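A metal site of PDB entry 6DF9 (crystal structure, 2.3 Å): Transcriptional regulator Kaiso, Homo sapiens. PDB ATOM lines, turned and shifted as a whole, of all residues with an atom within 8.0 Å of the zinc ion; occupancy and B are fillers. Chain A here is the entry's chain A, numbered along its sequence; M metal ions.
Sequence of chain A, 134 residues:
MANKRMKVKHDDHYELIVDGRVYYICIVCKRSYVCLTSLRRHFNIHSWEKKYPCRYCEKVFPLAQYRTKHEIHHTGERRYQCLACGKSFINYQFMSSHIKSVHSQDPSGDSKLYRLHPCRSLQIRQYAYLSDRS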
ATOM      1  N   PRO A  53      27.616 -21.244  10.696  1.00  0.00           N
ATOM      2  CA  PRO A  53      27.735 -21.128   9.235  1.00  0.00           C
ATOM      3  C   PRO A  53      26.869 -20.031   8.656  1.00  0.00           C
ATOM      4  O   PRO A  53      25.678 -20.016   8.966  1.00  0.00           O
ATOM      5  CB  PRO A  53      27.246 -22.487   8.735  1.00  0.00           C
ATOM      6  CG  PRO A  53      26.251 -22.911   9.769  1.00  0.00           C
ATOM      7  CD  PRO A  53      26.819 -22.418  11.085  1.00  0.00           C
ATOM      8  N   CYS A  54      27.434 -19.141   7.843  1.00  0.00           N
ATOM      9  CA  CYS A  54      26.614 -18.172   7.095  1.00  0.00           C
ATOM     10  C   CYS A  54      25.634 -18.939   6.218  1.00  0.00           C
ATOM     11  O   CYS A  54      26.024 -19.792   5.417  1.00  0.00           O
ATOM     12  CB  CYS A  54      27.481 -17.251   6.230  1.00  0.00           C
ATOM     13  SG  CYS A  54      26.547 -16.295   4.964  1.00  0.00           S
ATOM     14  N   ARG A  55      24.356 -18.653   6.388  1.00  0.00           N
ATOM     15  CA  ARG A  55      23.330 -19.322   5.590  1.00  0.00           C
ATOM     16  C   ARG A  55      23.249 -18.811   4.136  1.00  0.00           C
ATOM     17  O   ARG A  55      22.315 -19.169   3.415  1.00  0.00           O
ATOM     18  CB  ARG A  55      21.971 -19.172   6.257  1.00  0.00           C
ATOM     19  CG  ARG A  55      21.400 -17.775   6.168  1.00  0.00           C
ATOM     20  CD  ARG A  55      19.926 -17.752   6.514  1.00  0.00           C
ATOM     21  NE  ARG A  55      19.588 -16.578   7.311  1.00  0.00           N
ATOM     22  CZ  ARG A  55      18.588 -16.534   8.177  1.00  0.00           C
ATOM     23  NH1 ARG A  55      17.834 -17.605   8.369  1.00  0.00           N
ATOM     24  NH2 ARG A  55      18.357 -15.422   8.867  1.00  0.00           N
ATOM     25  N   TYR A  56      24.202 -17.980   3.713  1.00  0.00           N
ATOM     26  CA  TYR A  56      24.213 -17.481   2.339  1.00  0.00           C
ATOM     27  C   TYR A  56      25.468 -17.902   1.574  1.00  0.00           C
ATOM     28  O   TYR A  56      25.533 -17.770   0.357  1.00  0.00           O
ATOM     29  CB  TYR A  56      24.088 -15.954   2.288  1.00  0.00           C
ATOM     30  CG  TYR A  56      22.797 -15.419   2.874  1.00  0.00           C
ATOM     31  CD1 TYR A  56      21.650 -15.296   2.098  1.00  0.00           C
ATOM     32  CD2 TYR A  56      22.741 -15.010   4.198  1.00  0.00           C
ATOM     33  CE1 TYR A  56      20.474 -14.801   2.639  1.00  0.00           C
ATOM     34  CE2 TYR A  56      21.571 -14.520   4.745  1.00  0.00           C
ATOM     35  CZ  TYR A  56      20.443 -14.408   3.958  1.00  0.00           C
ATOM     36  OH  TYR A  56      19.296 -13.910   4.521  1.00  0.00           O
ATOM     37  N   CYS A  57      26.458 -18.411   2.288  1.00  0.00           N
ATOM     38  CA  CYS A  57      27.684 -18.858   1.643  1.00  0.00           C
ATOM     39  C   CYS A  57      28.419 -19.873   2.531  1.00  0.00           C
ATOM     40  O   CYS A  57      27.858 -20.372   3.508  1.00  0.00           O
ATOM     41  CB  CYS A  57      28.578 -17.652   1.317  1.00  0.00           C
ATOM     42  SG  CYS A  57      29.491 -16.970   2.738  1.00  0.00           S
ATOM     43  N   GLU A  58      29.677 -20.150   2.210  1.00  0.00           N
ATOM     44  CA  GLU A  58      30.422 -21.237   2.850  1.00  0.00           C
ATOM     45  C   GLU A  58      31.031 -20.861   4.206  1.00  0.00           C
ATOM     46  O   GLU A  58      31.438 -21.733   4.961  1.00  0.00           O
ATOM     47  CB  GLU A  58      31.533 -21.728   1.904  1.00  0.00           C
ATOM     48  CG  GLU A  58      32.660 -20.716   1.678  1.00  0.00           C
ATOM     49  CD  GLU A  58      32.250 -19.531   0.816  1.00  0.00           C
ATOM     50  OE1 GLU A  58      31.669 -19.749  -0.272  1.00  0.00           O
ATOM     51  OE2 GLU A  58      32.488 -18.366   1.215  1.00  0.00           O
ATOM     52  N   LYS A  59      31.096 -19.575   4.498  1.00  0.00           N
ATOM     53  CA  LYS A  59      31.849 -19.106   5.667  1.00  0.00           C
ATOM     54  C   LYS A  59      31.288 -19.578   7.007  1.00  0.00           C
ATOM     55  O   LYS A  59      30.069 -19.639   7.215  1.00  0.00           O
ATOM     56  CB  LYS A  59      31.942 -17.585   5.645  1.00  0.00           C
ATOM     57  CG  LYS A  59      32.823 -17.066   4.523  1.00  0.00           C
ATOM     58  CD  LYS A  59      33.063 -15.572   4.663  1.00  0.00           C
ATOM     59  CE  LYS A  59      34.020 -15.072   3.599  1.00  0.00           C
ATOM     60  NZ  LYS A  59      34.107 -13.576   3.644  1.00  0.00           N
ATOM     61  N   VAL A  60      32.183 -19.924   7.916  1.00  0.00           N
ATOM     62  CA  VAL A  60      31.788 -20.353   9.247  1.00  0.00           C
ATOM     63  C   VAL A  60      32.415 -19.430  10.287  1.00  0.00           C
ATOM     64  O   VAL A  60      33.539 -18.963  10.121  1.00  0.00           O
ATOM     65  CB  VAL A  60      32.171 -21.823   9.489  1.00  0.00           C
ATOM     66  CG1 VAL A  60      33.689 -21.980   9.555  1.00  0.00           C
ATOM     67  CG2 VAL A  60      31.509 -22.344  10.755  1.00  0.00           C
ATOM     68  N   PHE A  61      31.678 -19.151  11.359  1.00  0.00           N
ATOM     69  CA  PHE A  61      32.087 -18.191  12.377  1.00  0.00           C
ATOM     70  C   PHE A  61      32.096 -18.807  13.780  1.00  0.00           C
ATOM     71  O   PHE A  61      31.233 -19.632  14.090  1.00  0.00           O
ATOM     72  CB  PHE A  61      31.168 -16.969  12.344  1.00  0.00           C
ATOM     73  CG  PHE A  61      31.167 -16.247  11.024  1.00  0.00           C
ATOM     74  CD1 PHE A  61      30.240 -16.577  10.044  1.00  0.00           C
ATOM     75  CD2 PHE A  61      32.086 -15.242  10.763  1.00  0.00           C
ATOM     76  CE1 PHE A  61      30.242 -15.926   8.823  1.00  0.00           C
ATOM     77  CE2 PHE A  61      32.088 -14.589   9.560  1.00  0.00           C
ATOM     78  CZ  PHE A  61      31.166 -14.932   8.581  1.00  0.00           C
ATOM     79  N   ARG A  67      28.529 -14.018  12.661  1.00  0.00           N
ATOM     80  CA  ARG A  67      27.743 -14.507  11.542  1.00  0.00           C
ATOM     81  C   ARG A  67      26.621 -13.514  11.201  1.00  0.00           C
ATOM     82  O   ARG A  67      26.400 -13.195  10.044  1.00  0.00           O
ATOM     83  CB  ARG A  67      27.181 -15.892  11.837  1.00  0.00           C
ATOM     84  CG  ARG A  67      26.271 -16.377  10.709  1.00  0.00           C
ATOM     85  CD  ARG A  67      25.669 -17.722  10.995  1.00  0.00           C
ATOM     86  NE  ARG A  67      24.824 -17.704  12.177  1.00  0.00           N
ATOM     87  CZ  ARG A  67      24.281 -18.781  12.730  1.00  0.00           C
ATOM     88  NH1 ARG A  67      24.482 -19.975  12.194  1.00  0.00           N
ATOM     89  NH2 ARG A  67      23.514 -18.664  13.808  1.00  0.00           N
ATOM     90  N   HIS A  70      27.869 -10.582   9.398  1.00  0.00           N
ATOM     91  CA  HIS A  70      28.230 -11.028   8.074  1.00  0.00           C
ATOM     92  C   HIS A  70      26.998 -11.188   7.173  1.00  0.00           C
ATOM     93  O   HIS A  70      27.024 -10.851   5.989  1.00  0.00           O
ATOM     94  CB  HIS A  70      29.005 -12.351   8.145  1.00  0.00           C
ATOM     95  CG  HIS A  70      29.269 -12.963   6.806  1.00  0.00           C
ATOM     96  ND1 HIS A  70      30.211 -12.464   5.934  1.00  0.00           N
ATOM     97  CD2 HIS A  70      28.726 -14.038   6.191  1.00  0.00           C
ATOM     98  CE1 HIS A  70      30.237 -13.198   4.834  1.00  0.00           C
ATOM     99  NE2 HIS A  70      29.351 -14.163   4.967  1.00  0.00           N
ATOM    100  N   GLU A  71      25.919 -11.731   7.733  1.00  0.00           N
ATOM    101  CA  GLU A  71      24.734 -12.016   6.942  1.00  0.00           C
ATOM    102  C   GLU A  71      24.015 -10.730   6.543  1.00  0.00           C
ATOM    103  O   GLU A  71      23.371 -10.670   5.475  1.00  0.00           O
ATOM    104  CB  GLU A  71      23.809 -12.960   7.713  1.00  0.00           C
ATOM    105  CG  GLU A  71      24.272 -14.430   7.650  1.00  0.00           C
ATOM    106  CD  GLU A  71      23.401 -15.339   8.497  1.00  0.00           C
ATOM    107  OE1 GLU A  71      22.595 -14.803   9.284  1.00  0.00           O
ATOM    108  OE2 GLU A  71      23.520 -16.568   8.367  1.00  0.00           O
ATOM    109  N   ILE A  72      24.129  -9.698   7.370  1.00  0.00           N
ATOM    110  CA  ILE A  72      23.521  -8.407   7.031  1.00  0.00           C
ATOM    111  C   ILE A  72      24.234  -7.810   5.814  1.00  0.00           C
ATOM    112  O   ILE A  72      23.599  -7.152   4.982  1.00  0.00           O
ATOM    113  CB  ILE A  72      23.520  -7.449   8.247  1.00  0.00           C
ATOM    114  CG1 ILE A  72      22.278  -7.730   9.088  1.00  0.00           C
ATOM    115  CG2 ILE A  72      23.503  -5.981   7.816  1.00  0.00           C
ATOM    116  CD1 ILE A  72      22.364  -7.258  10.524  1.00  0.00           C
ATOM    117  N   HIS A  73      25.532  -8.073   5.676  1.00  0.00           N
ATOM    118  CA  HIS A  73      26.224  -7.741   4.433  1.00  0.00           C
ATOM    119  C   HIS A  73      25.591  -8.391   3.193  1.00  0.00           C
ATOM    120  O   HIS A  73      25.538  -7.776   2.140  1.00  0.00           O
ATOM    121  CB  HIS A  73      27.697  -8.145   4.497  1.00  0.00           C
ATOM    122  CG  HIS A  73      28.622  -7.013   4.793  1.00  0.00           C
ATOM    123  ND1 HIS A  73      28.913  -6.595   6.083  1.00  0.00           N
ATOM    124  CD2 HIS A  73      29.340  -6.208   3.972  1.00  0.00           C
ATOM    125  CE1 HIS A  73      29.759  -5.589   6.040  1.00  0.00           C
ATOM    126  NE2 HIS A  73      30.034  -5.332   4.776  1.00  0.00           N
ATOM    127  N   HIS A  74      25.146  -9.644   3.308  1.00  0.00           N
ATOM    128  CA  HIS A  74      24.544 -10.289   2.124  1.00  0.00           C
ATOM    129  C   HIS A  74      23.213  -9.630   1.700  1.00  0.00           C
ATOM    130  O   HIS A  74      22.892  -9.599   0.510  1.00  0.00           O
ATOM    131  CB  HIS A  74      24.309 -11.790   2.363  1.00  0.00           C
ATOM    132  CG  HIS A  74      25.535 -12.644   2.170  1.00  0.00           C
ATOM    133  ND1 HIS A  74      26.139 -12.818   0.940  1.00  0.00           N
ATOM    134  CD2 HIS A  74      26.236 -13.405   3.045  1.00  0.00           C
ATOM    135  CE1 HIS A  74      27.170 -13.634   1.080  1.00  0.00           C
ATOM    136  NE2 HIS A  74      27.253 -14.001   2.345  1.00  0.00           N
HETATM  137 ZN    ZN M   1      28.209 -15.362   3.703  1.00  0.00          ZN
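The side-chain sulfur (SG) of Cys 57 lies close to the backbone NH (N) of Lys 59, 3.5 Å away.
SG of Cys 57 lies close to OE2 of Glu 58.
The side-chain sulfur of Cys 54 lies close to the backbone NH of Tyr 56.
The backbone NH (N) of Cys 54 sits at hydrogen-bond distance from the backbone carbonyl oxygen (O) of Lys 59 (2.8 Å).
The zinc ion is bound by a ring nitrogen (NE2) of His 70 (2.1 Å), a ring nitrogen (NE2) of His 74 (2.1 Å), the side-chain sulfur of Cys 57 (2.3 Å) and the side-chain sulfur of Cys 54 (2.3 Å).
The zinc ion has four donor atoms within binding distance.
Of the 15 residues printed, 4 come within 4 Å of the zinc ion.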
